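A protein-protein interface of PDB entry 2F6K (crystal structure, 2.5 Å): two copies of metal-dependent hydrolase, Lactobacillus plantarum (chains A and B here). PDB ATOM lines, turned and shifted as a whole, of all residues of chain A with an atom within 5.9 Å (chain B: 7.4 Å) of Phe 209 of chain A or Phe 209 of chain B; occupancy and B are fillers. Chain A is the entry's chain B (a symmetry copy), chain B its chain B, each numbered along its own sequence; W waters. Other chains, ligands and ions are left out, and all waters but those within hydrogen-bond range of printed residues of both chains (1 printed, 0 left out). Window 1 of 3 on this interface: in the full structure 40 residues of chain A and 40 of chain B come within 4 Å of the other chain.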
ATOM      1  N   LEU A 174      22.983  -3.608 -16.513  1.00  0.00           N
ATOM      2  CA  LEU A 174      23.169  -4.894 -17.179  1.00  0.00           C
ATOM      3  C   LEU A 174      22.049  -5.212 -18.174  1.00  0.00           C
ATOM      4  O   LEU A 174      22.298  -5.788 -19.232  1.00  0.00           O
ATOM      5  CB  LEU A 174      23.275  -6.013 -16.130  1.00  0.00           C
ATOM      6  CG  LEU A 174      23.260  -7.472 -16.611  1.00  0.00           C
ATOM      7  CD1 LEU A 174      24.439  -7.744 -17.532  1.00  0.00           C
ATOM      8  CD2 LEU A 174      23.313  -8.395 -15.401  1.00  0.00           C
ATOM      9  N   PHE A 177      22.464  -3.673 -21.793  1.00  0.00           N
ATOM     10  CA  PHE A 177      23.411  -4.432 -22.606  1.00  0.00           C
ATOM     11  C   PHE A 177      22.860  -5.766 -23.083  1.00  0.00           C
ATOM     12  O   PHE A 177      23.054  -6.148 -24.239  1.00  0.00           O
ATOM     13  CB  PHE A 177      24.729  -4.657 -21.857  1.00  0.00           C
ATOM     14  CG  PHE A 177      25.663  -3.488 -21.923  1.00  0.00           C
ATOM     15  CD1 PHE A 177      27.033  -3.677 -21.846  1.00  0.00           C
ATOM     16  CD2 PHE A 177      25.174  -2.193 -22.084  1.00  0.00           C
ATOM     17  CE1 PHE A 177      27.908  -2.598 -21.933  1.00  0.00           C
ATOM     18  CE2 PHE A 177      26.038  -1.108 -22.171  1.00  0.00           C
ATOM     19  CZ  PHE A 177      27.406  -1.311 -22.097  1.00  0.00           C
ATOM     20  N   MET A 178      22.172  -6.484 -22.209  1.00  0.00           N
ATOM     21  CA  MET A 178      21.624  -7.760 -22.625  1.00  0.00           C
ATOM     22  C   MET A 178      20.620  -7.557 -23.752  1.00  0.00           C
ATOM     23  O   MET A 178      20.582  -8.339 -24.700  1.00  0.00           O
ATOM     24  CB  MET A 178      20.965  -8.477 -21.446  1.00  0.00           C
ATOM     25  CG  MET A 178      21.950  -8.807 -20.326  1.00  0.00           C
ATOM     26  SD  MET A 178      21.274 -10.024 -18.969  1.00  0.00           S
ATOM     27  CE  MET A 178      19.933  -8.882 -18.178  1.00  0.00           C
ATOM     28  N   THR A 181      22.313  -6.540 -27.101  1.00  0.00           N
ATOM     29  CA  THR A 181      22.963  -7.735 -27.635  1.00  0.00           C
ATOM     30  C   THR A 181      21.939  -8.661 -28.274  1.00  0.00           C
ATOM     31  O   THR A 181      22.121  -9.097 -29.411  1.00  0.00           O
ATOM     32  CB  THR A 181      23.719  -8.527 -26.552  1.00  0.00           C
ATOM     33  OG1 THR A 181      24.633  -7.660 -25.868  1.00  0.00           O
ATOM     34  CG2 THR A 181      24.519  -9.661 -27.197  1.00  0.00           C
ATOM     35  N   GLY A 207      28.525  -1.127 -28.704  1.00  0.00           N
ATOM     36  CA  GLY A 207      28.091  -2.456 -29.083  1.00  0.00           C
ATOM     37  C   GLY A 207      27.771  -3.420 -27.966  1.00  0.00           C
ATOM     38  O   GLY A 207      27.756  -4.625 -28.194  1.00  0.00           O
ATOM     39  N   ALA A 208      27.531  -2.909 -26.761  1.00  0.00           N
ATOM     40  CA  ALA A 208      27.186  -3.767 -25.629  1.00  0.00           C
ATOM     41  C   ALA A 208      28.117  -4.969 -25.479  1.00  0.00           C
ATOM     42  O   ALA A 208      29.309  -4.803 -25.241  1.00  0.00           O
ATOM     43  CB  ALA A 208      25.741  -4.245 -25.770  1.00  0.00           C
ATOM     44  N   PHE A 209      27.571  -6.175 -25.627  1.00  0.00           N
ATOM     45  CA  PHE A 209      28.356  -7.411 -25.487  1.00  0.00           C
ATOM     46  C   PHE A 209      28.824  -8.025 -26.801  1.00  0.00           C
ATOM     47  O   PHE A 209      29.371  -9.133 -26.807  1.00  0.00           O
ATOM     48  CB  PHE A 209      27.541  -8.481 -24.752  1.00  0.00           C
ATOM     49  CG  PHE A 209      27.199  -8.125 -23.337  1.00  0.00           C
ATOM     50  CD1 PHE A 209      26.001  -8.562 -22.772  1.00  0.00           C
ATOM     51  CD2 PHE A 209      28.060  -7.349 -22.572  1.00  0.00           C
ATOM     52  CE1 PHE A 209      25.663  -8.229 -21.463  1.00  0.00           C
ATOM     53  CE2 PHE A 209      27.734  -7.008 -21.262  1.00  0.00           C
ATOM     54  CZ  PHE A 209      26.529  -7.451 -20.705  1.00  0.00           C
ATOM     55  N   LEU A 210      28.607  -7.331 -27.911  1.00  0.00           N
ATOM     56  CA  LEU A 210      28.992  -7.874 -29.212  1.00  0.00           C
ATOM     57  C   LEU A 210      30.475  -8.232 -29.289  1.00  0.00           C
ATOM     58  O   LEU A 210      30.848  -9.251 -29.889  1.00  0.00           O
ATOM     59  CB  LEU A 210      28.612  -6.889 -30.335  1.00  0.00           C
ATOM     60  CG  LEU A 210      27.121  -6.497 -30.359  1.00  0.00           C
ATOM     61  CD1 LEU A 210      26.810  -5.660 -31.593  1.00  0.00           C
ATOM     62  CD2 LEU A 210      26.253  -7.749 -30.323  1.00  0.00           C
ATOM     63  N   GLY A 211      31.309  -7.404 -28.664  1.00  0.00           N
ATOM     64  CA  GLY A 211      32.741  -7.633 -28.669  1.00  0.00           C
ATOM     65  C   GLY A 211      33.152  -8.970 -28.087  1.00  0.00           C
ATOM     66  O   GLY A 211      34.290  -9.395 -28.259  1.00  0.00           O
ATOM     67  N   ILE A 212      32.237  -9.637 -27.392  1.00  0.00           N
ATOM     68  CA  ILE A 212      32.545 -10.933 -26.805  1.00  0.00           C
ATOM     69  C   ILE A 212      31.750 -12.084 -27.421  1.00  0.00           C
ATOM     70  O   ILE A 212      32.298 -13.168 -27.609  1.00  0.00           O
ATOM     71  CB  ILE A 212      32.315 -10.934 -25.272  1.00  0.00           C
ATOM     72  CG1 ILE A 212      33.369 -10.054 -24.592  1.00  0.00           C
ATOM     73  CG2 ILE A 212      32.360 -12.365 -24.733  1.00  0.00           C
ATOM     74  CD1 ILE A 212      33.311 -10.041 -23.059  1.00  0.00           C
ATOM     75  N   VAL A 213      30.475 -11.863 -27.740  1.00  0.00           N
ATOM     76  CA  VAL A 213      29.650 -12.934 -28.320  1.00  0.00           C
ATOM     77  C   VAL A 213      29.847 -13.213 -29.811  1.00  0.00           C
ATOM     78  O   VAL A 213      29.619 -14.341 -30.265  1.00  0.00           O
ATOM     79  CB  VAL A 213      28.134 -12.689 -28.119  1.00  0.00           C
ATOM     80  CG1 VAL A 213      27.801 -12.669 -26.652  1.00  0.00           C
ATOM     81  CG2 VAL A 213      27.721 -11.391 -28.790  1.00  0.00           C
ATOM     82  N   ASP A 214      30.242 -12.199 -30.578  1.00  0.00           N
ATOM     83  CA  ASP A 214      30.446 -12.391 -32.016  1.00  0.00           C
ATOM     84  C   ASP A 214      31.265 -13.647 -32.284  1.00  0.00           C
ATOM     85  O   ASP A 214      30.834 -14.542 -33.018  1.00  0.00           O
ATOM     86  CB  ASP A 214      31.167 -11.190 -32.634  1.00  0.00           C
ATOM     87  CG  ASP A 214      30.292  -9.963 -32.714  1.00  0.00           C
ATOM     88  OD1 ASP A 214      29.090 -10.072 -32.392  1.00  0.00           O
ATOM     89  OD2 ASP A 214      30.805  -8.892 -33.107  1.00  0.00           O
ATOM     90  N   GLN A 248      36.229  -2.112 -23.173  1.00  0.00           N
ATOM     91  CA  GLN A 248      35.199  -2.203 -24.208  1.00  0.00           C
ATOM     92  C   GLN A 248      35.536  -1.632 -25.590  1.00  0.00           C
ATOM     93  O   GLN A 248      35.447  -2.346 -26.596  1.00  0.00           O
ATOM     94  CB  GLN A 248      33.894  -1.575 -23.711  1.00  0.00           C
ATOM     95  CG  GLN A 248      32.673  -2.102 -24.450  1.00  0.00           C
ATOM     96  CD  GLN A 248      31.422  -1.297 -24.179  1.00  0.00           C
ATOM     97  OE1 GLN A 248      30.313  -1.742 -24.475  1.00  0.00           O
ATOM     98  NE2 GLN A 248      31.591  -0.101 -23.624  1.00  0.00           N
ATOM     99  N   LEU B 173      24.889 -20.346 -26.894  1.00  0.00           N
ATOM    100  CA  LEU B 173      25.474 -19.248 -27.645  1.00  0.00           C
ATOM    101  C   LEU B 173      25.378 -17.879 -26.969  1.00  0.00           C
ATOM    102  O   LEU B 173      26.317 -17.094 -27.045  1.00  0.00           O
ATOM    103  CB  LEU B 173      24.858 -19.184 -29.047  1.00  0.00           C
ATOM    104  CG  LEU B 173      25.021 -20.464 -29.877  1.00  0.00           C
ATOM    105  CD1 LEU B 173      24.474 -20.246 -31.292  1.00  0.00           C
ATOM    106  CD2 LEU B 173      26.484 -20.864 -29.914  1.00  0.00           C
ATOM    107  N   LEU B 174      24.261 -17.591 -26.309  1.00  0.00           N
ATOM    108  CA  LEU B 174      24.098 -16.298 -25.648  1.00  0.00           C
ATOM    109  C   LEU B 174      23.496 -16.423 -24.246  1.00  0.00           C
ATOM    110  O   LEU B 174      23.872 -15.687 -23.336  1.00  0.00           O
ATOM    111  CB  LEU B 174      23.227 -15.376 -26.517  1.00  0.00           C
ATOM    112  CG  LEU B 174      22.749 -14.044 -25.919  1.00  0.00           C
ATOM    113  CD1 LEU B 174      23.936 -13.164 -25.557  1.00  0.00           C
ATOM    114  CD2 LEU B 174      21.858 -13.336 -26.931  1.00  0.00           C
ATOM    115  N   GLY B 175      22.566 -17.357 -24.071  1.00  0.00           N
ATOM    116  CA  GLY B 175      21.938 -17.534 -22.772  1.00  0.00           C
ATOM    117  C   GLY B 175      22.915 -17.880 -21.659  1.00  0.00           C
ATOM    118  O   GLY B 175      22.877 -17.290 -20.573  1.00  0.00           O
ATOM    119  N   PHE B 176      23.791 -18.844 -21.916  1.00  0.00           N
ATOM    120  CA  PHE B 176      24.771 -19.236 -20.919  1.00  0.00           C
ATOM    121  C   PHE B 176      25.521 -18.003 -20.414  1.00  0.00           C
ATOM    122  O   PHE B 176      25.604 -17.769 -19.209  1.00  0.00           O
ATOM    123  CB  PHE B 176      25.756 -20.262 -21.501  1.00  0.00           C
ATOM    124  CG  PHE B 176      25.250 -21.701 -21.476  1.00  0.00           C
ATOM    125  CD1 PHE B 176      23.967 -22.005 -21.021  1.00  0.00           C
ATOM    126  CD2 PHE B 176      26.066 -22.750 -21.926  1.00  0.00           C
ATOM    127  CE1 PHE B 176      23.496 -23.332 -21.016  1.00  0.00           C
ATOM    128  CE2 PHE B 176      25.610 -24.076 -21.928  1.00  0.00           C
ATOM    129  CZ  PHE B 176      24.320 -24.370 -21.473  1.00  0.00           C
ATOM    130  N   PHE B 177      26.049 -17.199 -21.329  1.00  0.00           N
ATOM    131  CA  PHE B 177      26.786 -16.008 -20.914  1.00  0.00           C
ATOM    132  C   PHE B 177      25.944 -15.032 -20.107  1.00  0.00           C
ATOM    133  O   PHE B 177      26.409 -14.481 -19.107  1.00  0.00           O
ATOM    134  CB  PHE B 177      27.398 -15.287 -22.119  1.00  0.00           C
ATOM    135  CG  PHE B 177      28.693 -15.883 -22.580  1.00  0.00           C
ATOM    136  CD1 PHE B 177      29.646 -15.097 -23.206  1.00  0.00           C
ATOM    137  CD2 PHE B 177      28.971 -17.232 -22.369  1.00  0.00           C
ATOM    138  CE1 PHE B 177      30.862 -15.639 -23.612  1.00  0.00           C
ATOM    139  CE2 PHE B 177      30.181 -17.785 -22.772  1.00  0.00           C
ATOM    140  CZ  PHE B 177      31.128 -16.986 -23.393  1.00  0.00           C
ATOM    141  N   MET B 178      24.708 -14.808 -20.527  1.00  0.00           N
ATOM    142  CA  MET B 178      23.870 -13.888 -19.783  1.00  0.00           C
ATOM    143  C   MET B 178      23.652 -14.405 -18.367  1.00  0.00           C
ATOM    144  O   MET B 178      23.664 -13.630 -17.413  1.00  0.00           O
ATOM    145  CB  MET B 178      22.529 -13.685 -20.490  1.00  0.00           C
ATOM    146  CG  MET B 178      22.677 -13.064 -21.877  1.00  0.00           C
ATOM    147  SD  MET B 178      21.019 -12.446 -22.683  1.00  0.00           S
ATOM    148  CE  MET B 178      20.159 -14.154 -22.954  1.00  0.00           C
ATOM    149  N   ASP B 179      23.481 -15.717 -18.224  1.00  0.00           N
ATOM    150  CA  ASP B 179      23.246 -16.298 -16.903  1.00  0.00           C
ATOM    151  C   ASP B 179      24.475 -16.236 -15.991  1.00  0.00           C
ATOM    152  O   ASP B 179      24.374 -15.872 -14.819  1.00  0.00           O
ATOM    153  CB  ASP B 179      22.770 -17.746 -17.036  1.00  0.00           C
ATOM    154  CG  ASP B 179      21.668 -18.074 -16.057  1.00  0.00           C
ATOM    155  OD1 ASP B 179      20.632 -17.378 -16.094  1.00  0.00           O
ATOM    156  OD2 ASP B 179      21.831 -19.011 -15.249  1.00  0.00           O
ATOM    157  N   THR B 180      25.637 -16.588 -16.527  1.00  0.00           N
ATOM    158  CA  THR B 180      26.854 -16.547 -15.734  1.00  0.00           C
ATOM    159  C   THR B 180      27.094 -15.118 -15.280  1.00  0.00           C
ATOM    160  O   THR B 180      27.487 -14.885 -14.134  1.00  0.00           O
ATOM    161  CB  THR B 180      28.066 -17.027 -16.540  1.00  0.00           C
ATOM    162  OG1 THR B 180      27.844 -18.378 -16.965  1.00  0.00           O
ATOM    163  CG2 THR B 180      29.345 -16.944 -15.690  1.00  0.00           C
ATOM    164  N   THR B 181      26.854 -14.165 -16.175  1.00  0.00           N
ATOM    165  CA  THR B 181      27.040 -12.755 -15.839  1.00  0.00           C
ATOM    166  C   THR B 181      26.084 -12.338 -14.732  1.00  0.00           C
ATOM    167  O   THR B 181      26.505 -11.746 -13.737  1.00  0.00           O
ATOM    168  CB  THR B 181      26.813 -11.827 -17.047  1.00  0.00           C
ATOM    169  OG1 THR B 181      27.637 -12.247 -18.142  1.00  0.00           O
ATOM    170  CG2 THR B 181      27.191 -10.391 -16.681  1.00  0.00           C
ATOM    171  N   MET B 182      24.800 -12.654 -14.897  1.00  0.00           N
ATOM    172  CA  MET B 182      23.791 -12.312 -13.890  1.00  0.00           C
ATOM    173  C   MET B 182      24.100 -12.946 -12.533  1.00  0.00           C
ATOM    174  O   MET B 182      23.875 -12.332 -11.492  1.00  0.00           O
ATOM    175  CB  MET B 182      22.398 -12.763 -14.336  1.00  0.00           C
ATOM    176  CG  MET B 182      21.831 -12.023 -15.528  1.00  0.00           C
ATOM    177  SD  MET B 182      19.971 -12.518 -15.877  1.00  0.00           S
ATOM    178  CE  MET B 182      20.248 -14.157 -16.845  1.00  0.00           C
ATOM    179  N   PRO B 204      33.291 -20.083 -15.362  1.00  0.00           N
ATOM    180  CA  PRO B 204      33.560 -20.601 -16.706  1.00  0.00           C
ATOM    181  C   PRO B 204      33.621 -19.616 -17.862  1.00  0.00           C
ATOM    182  O   PRO B 204      33.372 -18.419 -17.710  1.00  0.00           O
ATOM    183  CB  PRO B 204      32.456 -21.632 -16.899  1.00  0.00           C
ATOM    184  CG  PRO B 204      31.317 -21.026 -16.161  1.00  0.00           C
ATOM    185  CD  PRO B 204      31.977 -20.549 -14.883  1.00  0.00           C
ATOM    186  N   HIS B 205      33.971 -20.160 -19.022  1.00  0.00           N
ATOM    187  CA  HIS B 205      34.079 -19.411 -20.268  1.00  0.00           C
ATOM    188  C   HIS B 205      34.683 -18.019 -20.136  1.00  0.00           C
ATOM    189  O   HIS B 205      34.073 -17.021 -20.517  1.00  0.00           O
ATOM    190  CB  HIS B 205      32.708 -19.330 -20.933  1.00  0.00           C
ATOM    191  CG  HIS B 205      32.002 -20.647 -20.994  1.00  0.00           C
ATOM    192  ND1 HIS B 205      30.900 -20.937 -20.218  1.00  0.00           N
ATOM    193  CD2 HIS B 205      32.261 -21.765 -21.713  1.00  0.00           C
ATOM    194  CE1 HIS B 205      30.512 -22.177 -20.456  1.00  0.00           C
ATOM    195  NE2 HIS B 205      31.321 -22.701 -21.360  1.00  0.00           N
ATOM    196  N   ALA B 206      35.890 -17.967 -19.586  1.00  0.00           N
ATOM    197  CA  ALA B 206      36.620 -16.718 -19.423  1.00  0.00           C
ATOM    198  C   ALA B 206      35.806 -15.576 -18.812  1.00  0.00           C
ATOM    199  O   ALA B 206      36.014 -14.404 -19.142  1.00  0.00           O
ATOM    200  CB  ALA B 206      37.207 -16.293 -20.774  1.00  0.00           C
ATOM    201  N   GLY B 207      34.872 -15.921 -17.935  1.00  0.00           N
ATOM    202  CA  GLY B 207      34.082 -14.906 -17.267  1.00  0.00           C
ATOM    203  C   GLY B 207      32.920 -14.323 -18.033  1.00  0.00           C
ATOM    204  O   GLY B 207      32.452 -13.242 -17.691  1.00  0.00           O
ATOM    205  N   ALA B 208      32.459 -15.014 -19.072  1.00  0.00           N
ATOM    206  CA  ALA B 208      31.318 -14.538 -19.854  1.00  0.00           C
ATOM    207  C   ALA B 208      31.433 -13.068 -20.250  1.00  0.00           C
ATOM    208  O   ALA B 208      32.343 -12.694 -20.985  1.00  0.00           O
ATOM    209  CB  ALA B 208      30.028 -14.763 -19.067  1.00  0.00           C
ATOM    210  N   PHE B 209      30.516 -12.238 -19.756  1.00  0.00           N
ATOM    211  CA  PHE B 209      30.505 -10.803 -20.080  1.00  0.00           C
ATOM    212  C   PHE B 209      31.144  -9.904 -19.027  1.00  0.00           C
ATOM    213  O   PHE B 209      31.067  -8.675 -19.132  1.00  0.00           O
ATOM    214  CB  PHE B 209      29.067 -10.311 -20.283  1.00  0.00           C
ATOM    215  CG  PHE B 209      28.367 -10.935 -21.451  1.00  0.00           C
ATOM    216  CD1 PHE B 209      26.991 -11.160 -21.408  1.00  0.00           C
ATOM    217  CD2 PHE B 209      29.074 -11.308 -22.587  1.00  0.00           C
ATOM    218  CE1 PHE B 209      26.328 -11.750 -22.480  1.00  0.00           C
ATOM    219  CE2 PHE B 209      28.423 -11.900 -23.666  1.00  0.00           C
ATOM    220  CZ  PHE B 209      27.043 -12.122 -23.612  1.00  0.00           C
ATOM    221  N   LEU B 210      31.760 -10.496 -18.011  1.00  0.00           N
ATOM    222  CA  LEU B 210      32.360  -9.700 -16.943  1.00  0.00           C
ATOM    223  C   LEU B 210      33.389  -8.695 -17.460  1.00  0.00           C
ATOM    224  O   LEU B 210      33.468  -7.561 -16.967  1.00  0.00           O
ATOM    225  CB  LEU B 210      32.987 -10.621 -15.879  1.00  0.00           C
ATOM    226  CG  LEU B 210      32.010 -11.648 -15.272  1.00  0.00           C
ATOM    227  CD1 LEU B 210      32.670 -12.395 -14.120  1.00  0.00           C
ATOM    228  CD2 LEU B 210      30.742 -10.944 -14.803  1.00  0.00           C
ATOM    229  N   GLY B 211      34.158  -9.111 -18.464  1.00  0.00           N
ATOM    230  CA  GLY B 211      35.176  -8.254 -19.038  1.00  0.00           C
ATOM    231  C   GLY B 211      34.640  -6.949 -19.590  1.00  0.00           C
ATOM    232  O   GLY B 211      35.409  -6.034 -19.869  1.00  0.00           O
ATOM    233  N   ILE B 212      33.325  -6.854 -19.759  1.00  0.00           N
ATOM    234  CA  ILE B 212      32.726  -5.633 -20.277  1.00  0.00           C
ATOM    235  C   ILE B 212      31.836  -4.916 -19.262  1.00  0.00           C
ATOM    236  O   ILE B 212      31.848  -3.688 -19.207  1.00  0.00           O
ATOM    237  CB  ILE B 212      31.899  -5.904 -21.560  1.00  0.00           C
ATOM    238  CG1 ILE B 212      32.841  -6.271 -22.712  1.00  0.00           C
ATOM    239  CG2 ILE B 212      31.052  -4.679 -21.909  1.00  0.00           C
ATOM    240  CD1 ILE B 212      32.156  -6.475 -24.069  1.00  0.00           C
ATOM    241  N   VAL B 213      31.073  -5.660 -18.462  1.00  0.00           N
ATOM    242  CA  VAL B 213      30.181  -5.030 -17.477  1.00  0.00           C
ATOM    243  C   VAL B 213      30.836  -4.532 -16.186  1.00  0.00           C
ATOM    244  O   VAL B 213      30.332  -3.593 -15.559  1.00  0.00           O
ATOM    245  CB  VAL B 213      29.022  -5.962 -17.045  1.00  0.00           C
ATOM    246  CG1 VAL B 213      28.152  -6.292 -18.228  1.00  0.00           C
ATOM    247  CG2 VAL B 213      29.576  -7.225 -16.408  1.00  0.00           C
ATOM    248  N   ASP B 214      31.933  -5.163 -15.772  1.00  0.00           N
ATOM    249  CA  ASP B 214      32.610  -4.744 -14.542  1.00  0.00           C
ATOM    250  C   ASP B 214      32.789  -3.232 -14.510  1.00  0.00           C
ATOM    251  O   ASP B 214      32.351  -2.561 -13.571  1.00  0.00           O
ATOM    252  CB  ASP B 214      33.985  -5.407 -14.420  1.00  0.00           C
ATOM    253  CG  ASP B 214      33.896  -6.881 -14.111  1.00  0.00           C
ATOM    254  OD1 ASP B 214      32.769  -7.371 -13.883  1.00  0.00           O
ATOM    255  OD2 ASP B 214      34.954  -7.549 -14.090  1.00  0.00           O
ATOM    256  N   ASP B 215      33.426  -2.705 -15.552  1.00  0.00           N
ATOM    257  CA  ASP B 215      33.680  -1.276 -15.664  1.00  0.00           C
ATOM    258  C   ASP B 215      32.401  -0.456 -15.599  1.00  0.00           C
ATOM    259  O   ASP B 215      32.406   0.675 -15.120  1.00  0.00           O
ATOM    260  CB  ASP B 215      34.427  -0.996 -16.965  1.00  0.00           C
ATOM    261  CG  ASP B 215      35.853  -1.528 -16.939  1.00  0.00           C
ATOM    262  OD1 ASP B 215      36.377  -1.877 -18.020  1.00  0.00           O
ATOM    263  OD2 ASP B 215      36.453  -1.585 -15.840  1.00  0.00           O
ATOM    264  N   ARG B 216      31.304  -1.041 -16.068  1.00  0.00           N
ATOM    265  CA  ARG B 216      30.008  -0.370 -16.067  1.00  0.00           C
ATOM    266  C   ARG B 216      29.317  -0.402 -14.704  1.00  0.00           C
ATOM    267  O   ARG B 216      28.610   0.536 -14.354  1.00  0.00           O
ATOM    268  CB  ARG B 216      29.090  -1.013 -17.113  1.00  0.00           C
ATOM    269  CG  ARG B 216      27.770  -0.282 -17.366  1.00  0.00           C
ATOM    270  CD  ARG B 216      26.976  -0.982 -18.474  1.00  0.00           C
ATOM    271  NE  ARG B 216      25.739  -0.283 -18.823  1.00  0.00           N
ATOM    272  CZ  ARG B 216      25.674   0.870 -19.487  1.00  0.00           C
ATOM    273  NH1 ARG B 216      26.779   1.480 -19.895  1.00  0.00           N
ATOM    274  NH2 ARG B 216      24.495   1.424 -19.733  1.00  0.00           N
ATOM    275  N   MET B 233      37.620  -9.754  -8.967  1.00  0.00           N
ATOM    276  CA  MET B 233      38.118 -10.367 -10.198  1.00  0.00           C
ATOM    277  C   MET B 233      39.516 -10.963  -9.994  1.00  0.00           C
ATOM    278  O   MET B 233      39.915 -11.889 -10.699  1.00  0.00           O
ATOM    279  CB  MET B 233      38.133  -9.345 -11.343  1.00  0.00           C
ATOM    280  CG  MET B 233      36.741  -8.939 -11.837  1.00  0.00           C
ATOM    281  SD  MET B 233      35.724 -10.412 -12.623  1.00  0.00           S
ATOM    282  CE  MET B 233      36.725 -10.610 -14.271  1.00  0.00           C
ATOM    283  N   GLN B 248      38.121 -12.121 -26.054  1.00  0.00           N
ATOM    284  CA  GLN B 248      37.708 -12.401 -24.679  1.00  0.00           C
ATOM    285  C   GLN B 248      38.816 -12.601 -23.637  1.00  0.00           C
ATOM    286  O   GLN B 248      38.843 -11.903 -22.617  1.00  0.00           O
ATOM    287  CB  GLN B 248      36.765 -13.607 -24.644  1.00  0.00           C
ATOM    288  CG  GLN B 248      35.880 -13.621 -23.408  1.00  0.00           C
ATOM    289  CD  GLN B 248      35.155 -14.934 -23.211  1.00  0.00           C
ATOM    290  OE1 GLN B 248      34.207 -15.017 -22.429  1.00  0.00           O
ATOM    291  NE2 GLN B 248      35.601 -15.972 -23.912  1.00  0.00           N
HETATM  292  O   HOH W   1      35.857  -0.829 -20.649  1.00  0.00           O
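Of the 13 printed residues of chain A, 8 touch a printed residue of chain B. Printed residues of chain A that touch a printed residue of chain B: Leu 174, Phe 177, Thr 181, Ala 208, Phe 209, Ile 212, Val 213 and Gln 248. Hydrophobic or aromatic side chains of chain A within 4 Å of the printed part of chain B: Leu 174, Phe 177, Phe 209, Ile 212 and Val 213. Along chain A the printed residues that touch a printed residue of chain B span positions 174 to 248. Of the 25 printed residues of chain B, 10 touch a printed residue of chain A. Among the printed residues, 14 pairs touch across the chains.
The side-chain hydroxyl (OG1) of Thr 181 of chain B sits close to the backbone NH (N) of Phe 209 of chain B (3.3 Å). The backbone carbonyl oxygen of Ala 208 of chain A sits close to the side-chain amide oxygen of Gln 248 of chain A, 3.3 Å away. The side-chain hydroxyl of Thr 181 of chain A lies close to the backbone NH of Phe 209 of chain A, at 3.3 Å. O of Ala 208 of chain B lies close to OE1 of Gln 248 of chain B. The side-chain hydroxyl of Thr 181 of chain A lies within hydrogen-bond range of the backbone carbonyl oxygen of Phe 177 of chain A (2.7 Å). The backbone carbonyl oxygen (O) of Phe 177 of chain B sits at hydrogen-bond distance from the side-chain hydroxyl (OG1) of Thr 181 of chain B.
Water W1 lies within hydrogen-bond range of the backbone NH of Gln 248 of chain A and the side-chain carboxylate of Asp 215 of chain B.
CD1 of Leu 174 of chain A touches CG2 of Thr 181 of chain B, at 3.9 Å. CG of Met 182 of chain B touches CD2 of Leu 174 of chain A, 3.9 Å away. CG2 of Ile 212 of chain B touches CE1 of Phe 177 of chain A, at 3.8 Å. Phe 177 of chain A touches Arg 216 of chain B. CD1 of Phe 209 of chain A touches CD1 of Phe 209 of chain B, at 3.1 Å. Ile 212 of chain A touches Phe 177 of chain B. CD1 of Ile 212 of chain A touches O of Ala 208 of chain B (3.5 Å). CG1 of Ile 212 of chain A touches CD1 of Ile 212 of chain B, 3.8 Å away. Gln 248 of chain B touches Ile 212 of chain A (CG to CG2, 3.97 Å). CG1 of Val 213 of chain A touches CE2 of Phe 209 of chain B, at 3.1 Å.
Printed residues of chain B within 4 Å of Phe 177 of chain A: Ile 212 (3.8 Å) and Arg 216 (3.4 Å). Gly 207 of chain A touches none of the printed residues of chain B. Printed residues of chain B within 4 Å of Ala 208 of chain A: Ile 212 (3.5 Å). Phe 209 of chain A touches just these residues of chain B: Phe 209 and Val 213. Printed residues of chain B within 4 Å of Ile 212 of chain A: Phe 177, Ala 208, Ile 212 and Gln 248. Of the printed residues of chain B, Gln 248 of chain A touches Ile 212. Leu 173 of chain B touches none of the printed residues of chain A. Printed residues of chain A within 4 Å of Thr 181 of chain B: Leu 174. Phe 209 of chain B touches two residues of chain A. The nearest residue of chain B that does not touch Phe 209 of chain A is Ile 212 of chain B (4.1 Å). The nearest printed residue of chain B that does not touch Ala 208 of chain A is Phe 209 of chain B (7.0 Å).
Ala 208 of chain A touches Ile 212 of chain B, and with the chains exchanged Ile 212 of chain A touches Ala 208 of chain B. Phe 209 of chain B touches its own counterpart, Phe 209 of chain A. Ile 212 of chain A touches its own counterpart, Ile 212 of chain B. Ile 212 of chain A touches Gln 248 of chain B, and with the chains exchanged Gln 248 of chain A touches Ile 212 of chain B. Of the 14 pairs that touch across the chains among the printed residues, 12 have their exchanged pair printed and touching as well.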
